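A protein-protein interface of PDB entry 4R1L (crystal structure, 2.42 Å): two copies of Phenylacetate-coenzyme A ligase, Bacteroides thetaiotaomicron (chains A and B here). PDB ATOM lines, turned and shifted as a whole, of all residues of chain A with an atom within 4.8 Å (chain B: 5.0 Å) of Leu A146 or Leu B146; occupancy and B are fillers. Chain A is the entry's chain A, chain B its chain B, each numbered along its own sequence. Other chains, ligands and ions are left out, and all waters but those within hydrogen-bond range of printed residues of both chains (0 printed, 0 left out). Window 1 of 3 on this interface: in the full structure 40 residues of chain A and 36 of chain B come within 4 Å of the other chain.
Printed residues of chain B within 4 Å of Leu A146: Leu B146 and Pro B161.
Printed residues of chain A within 4 Å of Leu B146: Leu A146 (3.7 Å), Gln A149 (3.9 Å) and Pro A161 (3.98 Å).
Printed residues of chain B within 4 Å of Arg A90: Gln B149 (3.7 Å).
Printed residues of chain A within 4 Å of Pro B161: Gly A140 and Leu A146.
Of the printed residues of chain B, Tyr A150 touches Gln B149 (3.98 Å) and Tyr B150 (3.3 Å).
Of the printed residues of chain B, Pro A161 touches Gly B140 and Leu B146.
Of the printed residues of chain B, Gln A149 touches Arg B90 and Leu B146.
Gly B145 touches none of the printed residues of chain A.
The nearest printed residue of chain A that does not touch Leu B146 is Tyr A139 (4.5 Å).
Among the printed residues, pairs that only touch across the chains: Pro A161 with Gly B140, Gly A140 with Pro B161, Tyr A150 with Tyr B150, Tyr A139 with Tyr B139, Arg A90 with Gln B149, Gln A149 with Arg B90, Leu A146 with Leu B146, Gln A149 with Leu B146, Tyr A139 with Gly B140, Leu A146 with Pro B161, Tyr A150 with Gln B149 and Pro A161 with Leu B146.
NH1 of Arg A90 is in hydrogen-bond range of NE2 of His A92, 3.1 Å away.
NH2 of Arg A90 sits close to OH of Tyr A150 (3.2 Å).
The side-chain amide oxygen (OE1) of Gln A149 sits at hydrogen-bond distance from the side-chain hydroxyl (OH) of Tyr A139, 2.7 Å away.
The guanidinium group (NH1) of Arg B90 is in hydrogen-bond range of a ring nitrogen (NE2) of His B92, 2.9 Å away.
OH of Tyr B150 lies close to NH2 of Arg B90, 3.2 Å away.
OE1 of Gln B149 is in hydrogen-bond range of OH of Tyr B139, 2.7 Å away.
Gly A140 touches Pro B161, and with the chains exchanged Pro A161 touches Gly B140.
Leu A146 touches its own counterpart, Leu B146.
Tyr A150 touches Gln B149, but with the chains exchanged Gln A149 does not touch Tyr B150 (4.1 Å).
Tyr A150 touches its own counterpart, Tyr B150.
Positions printed for both chains: 90, 92, 139, 140, 142, 143, 144, 145, 146, 147, 148, 149, 150, 151 and 161.
Of the 12 pairs that touch across the chains among the printed residues, 9 have their exchanged pair printed and touching as well.
Printed residues of chain A that touch a printed residue of chain B: Arg A90, Tyr A139, Gly A140, Leu A146, Gln A149, Tyr A150 and Pro A161.
Of the 16 printed residues of chain B, 7 touch a printed residue of chain A.
Printed residues of chain B that touch a printed residue of chain A: Arg B90, Tyr B139, Gly B140, Leu B146, Gln B149, Tyr B150 and Pro B161.
Hydrophobic or aromatic side chains of chain B that line the printed part of chain A: Tyr B139, Leu B146, Tyr B150 and Pro B161.
Among the printed residues, 12 pairs touch across the chains.
Among the printed residues, no Asp or Glu carboxylate lies within 4 Å of a Lys or Arg side-chain nitrogen of the other chain.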
ATOM      1  N   ARG A  90      22.960  13.341   7.829  1.00  0.00           N
ATOM      2  CA  ARG A  90      24.328  13.749   8.154  1.00  0.00           C
ATOM      3  C   ARG A  90      24.871  13.087   9.401  1.00  0.00           C
ATOM      4  O   ARG A  90      24.143  12.880  10.363  1.00  0.00           O
ATOM      5  CB  ARG A  90      24.486  15.278   8.347  1.00  0.00           C
ATOM      6  CG  ARG A  90      25.961  15.678   8.029  1.00  0.00           C
ATOM      7  CD  ARG A  90      26.292  17.110   8.247  1.00  0.00           C
ATOM      8  NE  ARG A  90      25.538  18.016   7.384  1.00  0.00           N
ATOM      9  CZ  ARG A  90      25.370  19.305   7.653  1.00  0.00           C
ATOM     10  NH1 ARG A  90      25.909  19.841   8.745  1.00  0.00           N
ATOM     11  NH2 ARG A  90      24.653  20.064   6.850  1.00  0.00           N
ATOM     12  N   HIS A  92      28.176  13.802  12.099  1.00  0.00           N
ATOM     13  CA  HIS A  92      29.283  14.599  12.601  1.00  0.00           C
ATOM     14  C   HIS A  92      30.014  13.720  13.566  1.00  0.00           C
ATOM     15  O   HIS A  92      29.430  13.226  14.527  1.00  0.00           O
ATOM     16  CB  HIS A  92      28.900  15.971  13.198  1.00  0.00           C
ATOM     17  CG  HIS A  92      28.646  17.001  12.138  1.00  0.00           C
ATOM     18  ND1 HIS A  92      29.696  17.601  11.446  1.00  0.00           N
ATOM     19  CD2 HIS A  92      27.477  17.479  11.650  1.00  0.00           C
ATOM     20  CE1 HIS A  92      29.134  18.432  10.579  1.00  0.00           C
ATOM     21  NE2 HIS A  92      27.803  18.403  10.668  1.00  0.00           N
ATOM     22  N   TYR A 139      35.945  23.164   7.787  1.00  0.00           N
ATOM     23  CA  TYR A 139      34.718  22.546   7.301  1.00  0.00           C
ATOM     24  C   TYR A 139      34.857  21.015   7.508  1.00  0.00           C
ATOM     25  O   TYR A 139      35.471  20.597   8.509  1.00  0.00           O
ATOM     26  CB  TYR A 139      34.442  22.974   5.845  1.00  0.00           C
ATOM     27  CG  TYR A 139      33.754  24.325   5.773  1.00  0.00           C
ATOM     28  CD1 TYR A 139      34.363  25.471   6.287  1.00  0.00           C
ATOM     29  CD2 TYR A 139      32.492  24.457   5.201  1.00  0.00           C
ATOM     30  CE1 TYR A 139      33.714  26.704   6.278  1.00  0.00           C
ATOM     31  CE2 TYR A 139      31.857  25.692   5.134  1.00  0.00           C
ATOM     32  CZ  TYR A 139      32.468  26.812   5.689  1.00  0.00           C
ATOM     33  OH  TYR A 139      31.835  28.028   5.678  1.00  0.00           O
ATOM     34  N   GLY A 140      34.254  20.201   6.644  1.00  0.00           N
ATOM     35  CA  GLY A 140      34.287  18.746   6.798  1.00  0.00           C
ATOM     36  C   GLY A 140      33.478  18.298   8.002  1.00  0.00           C
ATOM     37  O   GLY A 140      32.308  18.697   8.145  1.00  0.00           O
ATOM     38  N   PHE A 142      34.005  19.138  11.178  1.00  0.00           N
ATOM     39  CA  PHE A 142      33.897  20.227  12.158  1.00  0.00           C
ATOM     40  C   PHE A 142      32.566  20.922  12.020  1.00  0.00           C
ATOM     41  O   PHE A 142      32.237  21.394  10.934  1.00  0.00           O
ATOM     42  CB  PHE A 142      35.030  21.242  11.993  1.00  0.00           C
ATOM     43  CG  PHE A 142      36.424  20.732  12.214  1.00  0.00           C
ATOM     44  CD1 PHE A 142      36.870  20.418  13.488  1.00  0.00           C
ATOM     45  CD2 PHE A 142      37.335  20.680  11.166  1.00  0.00           C
ATOM     46  CE1 PHE A 142      38.193  20.013  13.700  1.00  0.00           C
ATOM     47  CE2 PHE A 142      38.656  20.270  11.382  1.00  0.00           C
ATOM     48  CZ  PHE A 142      39.077  19.950  12.649  1.00  0.00           C
ATOM     49  N   THR A 143      31.812  21.007  13.114  1.00  0.00           N
ATOM     50  CA  THR A 143      30.463  21.573  13.098  1.00  0.00           C
ATOM     51  C   THR A 143      30.477  23.108  12.874  1.00  0.00           C
ATOM     52  O   THR A 143      29.502  23.597  12.330  1.00  0.00           O
ATOM     53  CB  THR A 143      29.693  21.212  14.356  1.00  0.00           C
ATOM     54  OG1 THR A 143      30.453  21.533  15.524  1.00  0.00           O
ATOM     55  CG2 THR A 143      29.330  19.758  14.372  1.00  0.00           C
ATOM     56  N   GLY A 144      31.555  23.824  13.221  1.00  0.00           N
ATOM     57  CA  GLY A 144      31.669  25.266  12.971  1.00  0.00           C
ATOM     58  C   GLY A 144      31.605  25.638  11.490  1.00  0.00           C
ATOM     59  O   GLY A 144      31.135  26.726  11.133  1.00  0.00           O
ATOM     60  N   GLY A 145      32.052  24.709  10.627  1.00  0.00           N
ATOM     61  CA  GLY A 145      32.051  24.831   9.174  1.00  0.00           C
ATOM     62  C   GLY A 145      30.657  24.890   8.591  1.00  0.00           C
ATOM     63  O   GLY A 145      30.156  25.977   8.277  1.00  0.00           O
ATOM     64  N   LEU A 146      30.018  23.726   8.467  1.00  0.00           N
ATOM     65  CA  LEU A 146      28.666  23.572   7.919  1.00  0.00           C
ATOM     66  C   LEU A 146      27.586  24.235   8.814  1.00  0.00           C
ATOM     67  O   LEU A 146      26.582  24.702   8.277  1.00  0.00           O
ATOM     68  CB  LEU A 146      28.342  22.084   7.730  1.00  0.00           C
ATOM     69  CG  LEU A 146      29.043  21.406   6.539  1.00  0.00           C
ATOM     70  CD1 LEU A 146      28.993  19.870   6.664  1.00  0.00           C
ATOM     71  CD2 LEU A 146      28.441  21.859   5.219  1.00  0.00           C
ATOM     72  N   GLY A 147      27.821  24.321  10.118  1.00  0.00           N
ATOM     73  CA  GLY A 147      26.931  24.960  11.088  1.00  0.00           C
ATOM     74  C   GLY A 147      26.655  26.425  10.792  1.00  0.00           C
ATOM     75  O   GLY A 147      25.483  26.839  10.689  1.00  0.00           O
ATOM     76  N   PHE A 148      27.745  27.225  10.699  1.00  0.00           N
ATOM     77  CA  PHE A 148      27.658  28.642  10.381  1.00  0.00           C
ATOM     78  C   PHE A 148      27.312  28.836   8.914  1.00  0.00           C
ATOM     79  O   PHE A 148      26.550  29.755   8.615  1.00  0.00           O
ATOM     80  CB  PHE A 148      28.932  29.406  10.722  1.00  0.00           C
ATOM     81  CG  PHE A 148      28.991  29.789  12.168  1.00  0.00           C
ATOM     82  CD1 PHE A 148      28.239  30.851  12.652  1.00  0.00           C
ATOM     83  CD2 PHE A 148      29.808  29.094  13.055  1.00  0.00           C
ATOM     84  CE1 PHE A 148      28.293  31.205  13.998  1.00  0.00           C
ATOM     85  CE2 PHE A 148      29.895  29.477  14.389  1.00  0.00           C
ATOM     86  CZ  PHE A 148      29.137  30.530  14.857  1.00  0.00           C
ATOM     87  N   GLN A 149      27.834  27.972   8.007  1.00  0.00           N
ATOM     88  CA  GLN A 149      27.484  28.023   6.589  1.00  0.00           C
ATOM     89  C   GLN A 149      25.936  28.021   6.392  1.00  0.00           C
ATOM     90  O   GLN A 149      25.409  28.966   5.810  1.00  0.00           O
ATOM     91  CB  GLN A 149      28.118  26.856   5.819  1.00  0.00           C
ATOM     92  CG  GLN A 149      27.992  26.986   4.288  1.00  0.00           C
ATOM     93  CD  GLN A 149      28.625  28.260   3.791  1.00  0.00           C
ATOM     94  OE1 GLN A 149      29.716  28.654   4.203  1.00  0.00           O
ATOM     95  NE2 GLN A 149      27.919  28.958   2.953  1.00  0.00           N
ATOM     96  N   TYR A 150      25.231  27.006   6.934  1.00  0.00           N
ATOM     97  CA  TYR A 150      23.774  26.848   6.846  1.00  0.00           C
ATOM     98  C   TYR A 150      23.050  27.953   7.588  1.00  0.00           C
ATOM     99  O   TYR A 150      22.040  28.458   7.080  1.00  0.00           O
ATOM    100  CB  TYR A 150      23.341  25.476   7.397  1.00  0.00           C
ATOM    101  CG  TYR A 150      23.540  24.327   6.420  1.00  0.00           C
ATOM    102  CD1 TYR A 150      24.760  24.139   5.769  1.00  0.00           C
ATOM    103  CD2 TYR A 150      22.542  23.378   6.216  1.00  0.00           C
ATOM    104  CE1 TYR A 150      24.963  23.071   4.899  1.00  0.00           C
ATOM    105  CE2 TYR A 150      22.734  22.301   5.343  1.00  0.00           C
ATOM    106  CZ  TYR A 150      23.941  22.166   4.672  1.00  0.00           C
ATOM    107  OH  TYR A 150      24.181  21.118   3.815  1.00  0.00           O
ATOM    108  N   GLY A 151      23.580  28.324   8.766  1.00  0.00           N
ATOM    109  CA  GLY A 151      23.041  29.383   9.610  1.00  0.00           C
ATOM    110  C   GLY A 151      23.029  30.727   8.904  1.00  0.00           C
ATOM    111  O   GLY A 151      21.995  31.394   8.825  1.00  0.00           O
ATOM    112  N   PRO A 161      32.762  30.915   2.322  1.00  0.00           N
ATOM    113  CA  PRO A 161      33.234  29.694   3.016  1.00  0.00           C
ATOM    114  C   PRO A 161      34.771  29.550   2.917  1.00  0.00           C
ATOM    115  O   PRO A 161      35.285  28.619   2.269  1.00  0.00           O
ATOM    116  CB  PRO A 161      32.504  28.577   2.265  1.00  0.00           C
ATOM    117  CG  PRO A 161      32.349  29.112   0.848  1.00  0.00           C
ATOM    118  CD  PRO A 161      32.175  30.603   0.992  1.00  0.00           C
ATOM    119  N   ARG B  90      26.218  33.201  -1.507  1.00  0.00           N
ATOM    120  CA  ARG B  90      27.491  32.465  -1.511  1.00  0.00           C
ATOM    121  C   ARG B  90      28.443  32.916  -2.588  1.00  0.00           C
ATOM    122  O   ARG B  90      28.033  33.253  -3.689  1.00  0.00           O
ATOM    123  CB  ARG B  90      27.307  30.940  -1.694  1.00  0.00           C
ATOM    124  CG  ARG B  90      28.515  30.202  -1.095  1.00  0.00           C
ATOM    125  CD  ARG B  90      28.497  28.734  -1.298  1.00  0.00           C
ATOM    126  NE  ARG B  90      27.401  28.071  -0.590  1.00  0.00           N
ATOM    127  CZ  ARG B  90      27.004  26.845  -0.871  1.00  0.00           C
ATOM    128  NH1 ARG B  90      27.589  26.156  -1.847  1.00  0.00           N
ATOM    129  NH2 ARG B  90      26.005  26.300  -0.203  1.00  0.00           N
ATOM    130  N   HIS B  92      31.989  31.259  -4.353  1.00  0.00           N
ATOM    131  CA  HIS B  92      32.942  30.168  -4.553  1.00  0.00           C
ATOM    132  C   HIS B  92      34.103  30.676  -5.371  1.00  0.00           C
ATOM    133  O   HIS B  92      33.977  31.714  -6.017  1.00  0.00           O
ATOM    134  CB  HIS B  92      32.327  28.926  -5.208  1.00  0.00           C
ATOM    135  CG  HIS B  92      31.566  28.048  -4.259  1.00  0.00           C
ATOM    136  ND1 HIS B  92      32.224  27.253  -3.327  1.00  0.00           N
ATOM    137  CD2 HIS B  92      30.239  27.803  -4.183  1.00  0.00           C
ATOM    138  CE1 HIS B  92      31.278  26.566  -2.706  1.00  0.00           C
ATOM    139  NE2 HIS B  92      30.069  26.859  -3.182  1.00  0.00           N
ATOM    140  N   TRP B 114      21.606  24.229  -8.412  1.00  0.00           N
ATOM    141  CA  TRP B 114      22.861  23.495  -8.391  1.00  0.00           C
ATOM    142  C   TRP B 114      22.663  22.188  -7.634  1.00  0.00           C
ATOM    143  O   TRP B 114      23.004  21.139  -8.175  1.00  0.00           O
ATOM    144  CB  TRP B 114      23.953  24.370  -7.764  1.00  0.00           C
ATOM    145  CG  TRP B 114      25.301  23.741  -7.509  1.00  0.00           C
ATOM    146  CD1 TRP B 114      25.845  22.644  -8.118  1.00  0.00           C
ATOM    147  CD2 TRP B 114      26.339  24.305  -6.700  1.00  0.00           C
ATOM    148  NE1 TRP B 114      27.128  22.439  -7.667  1.00  0.00           N
ATOM    149  CE2 TRP B 114      27.457  23.445  -6.791  1.00  0.00           C
ATOM    150  CE3 TRP B 114      26.429  25.457  -5.900  1.00  0.00           C
ATOM    151  CZ2 TRP B 114      28.657  23.710  -6.124  1.00  0.00           C
ATOM    152  CZ3 TRP B 114      27.619  25.719  -5.240  1.00  0.00           C
ATOM    153  CH2 TRP B 114      28.722  24.862  -5.371  1.00  0.00           C
ATOM    154  N   TYR B 139      36.463  21.021   1.237  1.00  0.00           N
ATOM    155  CA  TYR B 139      35.296  21.864   1.458  1.00  0.00           C
ATOM    156  C   TYR B 139      35.754  23.341   1.341  1.00  0.00           C
ATOM    157  O   TYR B 139      36.584  23.632   0.478  1.00  0.00           O
ATOM    158  CB  TYR B 139      34.596  21.506   2.787  1.00  0.00           C
ATOM    159  CG  TYR B 139      33.641  20.336   2.628  1.00  0.00           C
ATOM    160  CD1 TYR B 139      34.099  19.084   2.214  1.00  0.00           C
ATOM    161  CD2 TYR B 139      32.290  20.460   2.944  1.00  0.00           C
ATOM    162  CE1 TYR B 139      33.230  18.009   2.046  1.00  0.00           C
ATOM    163  CE2 TYR B 139      31.417  19.381   2.820  1.00  0.00           C
ATOM    164  CZ  TYR B 139      31.889  18.159   2.359  1.00  0.00           C
ATOM    165  OH  TYR B 139      31.047  17.090   2.191  1.00  0.00           O
ATOM    166  N   GLY B 140      35.163  24.253   2.085  1.00  0.00           N
ATOM    167  CA  GLY B 140      35.530  25.650   1.968  1.00  0.00           C
ATOM    168  C   GLY B 140      35.076  26.254   0.651  1.00  0.00           C
ATOM    169  O   GLY B 140      33.917  26.108   0.237  1.00  0.00           O
ATOM    170  N   PHE B 142      36.135  25.406  -2.373  1.00  0.00           N
ATOM    171  CA  PHE B 142      36.044  24.351  -3.402  1.00  0.00           C
ATOM    172  C   PHE B 142      34.606  23.940  -3.590  1.00  0.00           C
ATOM    173  O   PHE B 142      33.958  23.540  -2.631  1.00  0.00           O
ATOM    174  CB  PHE B 142      36.904  23.103  -3.042  1.00  0.00           C
ATOM    175  CG  PHE B 142      38.385  23.365  -2.877  1.00  0.00           C
ATOM    176  CD1 PHE B 142      39.172  23.744  -3.968  1.00  0.00           C
ATOM    177  CD2 PHE B 142      39.005  23.210  -1.635  1.00  0.00           C
ATOM    178  CE1 PHE B 142      40.537  24.030  -3.808  1.00  0.00           C
ATOM    179  CE2 PHE B 142      40.378  23.465  -1.482  1.00  0.00           C
ATOM    180  CZ  PHE B 142      41.134  23.883  -2.570  1.00  0.00           C
ATOM    181  N   THR B 143      34.111  23.993  -4.826  1.00  0.00           N
ATOM    182  CA  THR B 143      32.710  23.694  -5.125  1.00  0.00           C
ATOM    183  C   THR B 143      32.346  22.196  -4.907  1.00  0.00           C
ATOM    184  O   THR B 143      31.172  21.915  -4.711  1.00  0.00           O
ATOM    185  CB  THR B 143      32.379  24.092  -6.562  1.00  0.00           C
ATOM    186  OG1 THR B 143      33.104  23.262  -7.452  1.00  0.00           O
ATOM    187  CG2 THR B 143      32.647  25.565  -6.843  1.00  0.00           C
ATOM    188  N   GLY B 144      33.323  21.280  -4.969  1.00  0.00           N
ATOM    189  CA  GLY B 144      33.094  19.851  -4.766  1.00  0.00           C
ATOM    190  C   GLY B 144      32.604  19.481  -3.377  1.00  0.00           C
ATOM    191  O   GLY B 144      31.863  18.510  -3.208  1.00  0.00           O
ATOM    192  N   GLY B 145      33.038  20.251  -2.382  1.00  0.00           N
ATOM    193  CA  GLY B 145      32.670  20.088  -0.983  1.00  0.00           C
ATOM    194  C   GLY B 145      31.205  20.366  -0.765  1.00  0.00           C
ATOM    195  O   GLY B 145      30.425  19.428  -0.629  1.00  0.00           O
ATOM    196  N   LEU B 146      30.809  21.651  -0.763  1.00  0.00           N
ATOM    197  CA  LEU B 146      29.423  22.076  -0.533  1.00  0.00           C
ATOM    198  C   LEU B 146      28.487  21.628  -1.674  1.00  0.00           C
ATOM    199  O   LEU B 146      27.289  21.403  -1.430  1.00  0.00           O
ATOM    200  CB  LEU B 146      29.372  23.608  -0.364  1.00  0.00           C
ATOM    201  CG  LEU B 146      29.905  24.148   0.994  1.00  0.00           C
ATOM    202  CD1 LEU B 146      30.161  25.637   0.955  1.00  0.00           C
ATOM    203  CD2 LEU B 146      28.940  23.831   2.138  1.00  0.00           C
ATOM    204  N   GLY B 147      29.062  21.440  -2.875  1.00  0.00           N
ATOM    205  CA  GLY B 147      28.363  20.981  -4.073  1.00  0.00           C
ATOM    206  C   GLY B 147      27.743  19.610  -3.922  1.00  0.00           C
ATOM    207  O   GLY B 147      26.526  19.465  -4.076  1.00  0.00           O
ATOM    208  N   PHE B 148      28.565  18.599  -3.568  1.00  0.00           N
ATOM    209  CA  PHE B 148      28.033  17.252  -3.311  1.00  0.00           C
ATOM    210  C   PHE B 148      27.319  17.164  -1.939  1.00  0.00           C
ATOM    211  O   PHE B 148      26.377  16.380  -1.806  1.00  0.00           O
ATOM    212  CB  PHE B 148      29.133  16.189  -3.395  1.00  0.00           C
ATOM    213  CG  PHE B 148      29.360  15.764  -4.832  1.00  0.00           C
ATOM    214  CD1 PHE B 148      28.467  14.913  -5.472  1.00  0.00           C
ATOM    215  CD2 PHE B 148      30.448  16.244  -5.552  1.00  0.00           C
ATOM    216  CE1 PHE B 148      28.656  14.556  -6.815  1.00  0.00           C
ATOM    217  CE2 PHE B 148      30.643  15.873  -6.885  1.00  0.00           C
ATOM    218  CZ  PHE B 148      29.746  15.029  -7.510  1.00  0.00           C
ATOM    219  N   GLN B 149      27.718  17.989  -0.953  1.00  0.00           N
ATOM    220  CA  GLN B 149      27.079  18.006   0.361  1.00  0.00           C
ATOM    221  C   GLN B 149      25.574  18.321   0.234  1.00  0.00           C
ATOM    222  O   GLN B 149      24.757  17.509   0.656  1.00  0.00           O
ATOM    223  CB  GLN B 149      27.774  19.019   1.297  1.00  0.00           C
ATOM    224  CG  GLN B 149      27.312  18.910   2.743  1.00  0.00           C
ATOM    225  CD  GLN B 149      27.527  17.521   3.304  1.00  0.00           C
ATOM    226  OE1 GLN B 149      28.557  16.870   3.090  1.00  0.00           O
ATOM    227  NE2 GLN B 149      26.537  17.017   4.009  1.00  0.00           N
ATOM    228  N   TYR B 150      25.218  19.449  -0.407  1.00  0.00           N
ATOM    229  CA  TYR B 150      23.837  19.897  -0.644  1.00  0.00           C
ATOM    230  C   TYR B 150      23.071  18.961  -1.561  1.00  0.00           C
ATOM    231  O   TYR B 150      21.913  18.679  -1.271  1.00  0.00           O
ATOM    232  CB  TYR B 150      23.808  21.310  -1.242  1.00  0.00           C
ATOM    233  CG  TYR B 150      24.007  22.395  -0.209  1.00  0.00           C
ATOM    234  CD1 TYR B 150      25.091  22.358   0.673  1.00  0.00           C
ATOM    235  CD2 TYR B 150      23.155  23.498  -0.153  1.00  0.00           C
ATOM    236  CE1 TYR B 150      25.289  23.358   1.620  1.00  0.00           C
ATOM    237  CE2 TYR B 150      23.345  24.511   0.794  1.00  0.00           C
ATOM    238  CZ  TYR B 150      24.407  24.429   1.684  1.00  0.00           C
ATOM    239  OH  TYR B 150      24.621  25.433   2.598  1.00  0.00           O
ATOM    240  N   GLY B 151      23.687  18.504  -2.652  1.00  0.00           N
ATOM    241  CA  GLY B 151      23.063  17.564  -3.580  1.00  0.00           C
ATOM    242  C   GLY B 151      22.712  16.231  -2.929  1.00  0.00           C
ATOM    243  O   GLY B 151      21.586  15.752  -3.081  1.00  0.00           O
ATOM    244  N   PRO B 161      30.543  14.121   5.658  1.00  0.00           N
ATOM    245  CA  PRO B 161      31.398  15.203   5.098  1.00  0.00           C
ATOM    246  C   PRO B 161      32.860  15.035   5.534  1.00  0.00           C
ATOM    247  O   PRO B 161      33.383  15.838   6.312  1.00  0.00           O
ATOM    248  CB  PRO B 161      30.770  16.474   5.681  1.00  0.00           C
ATOM    249  CG  PRO B 161      30.171  16.013   7.012  1.00  0.00           C
ATOM    250  CD  PRO B 161      29.741  14.585   6.814  1.00  0.00           C
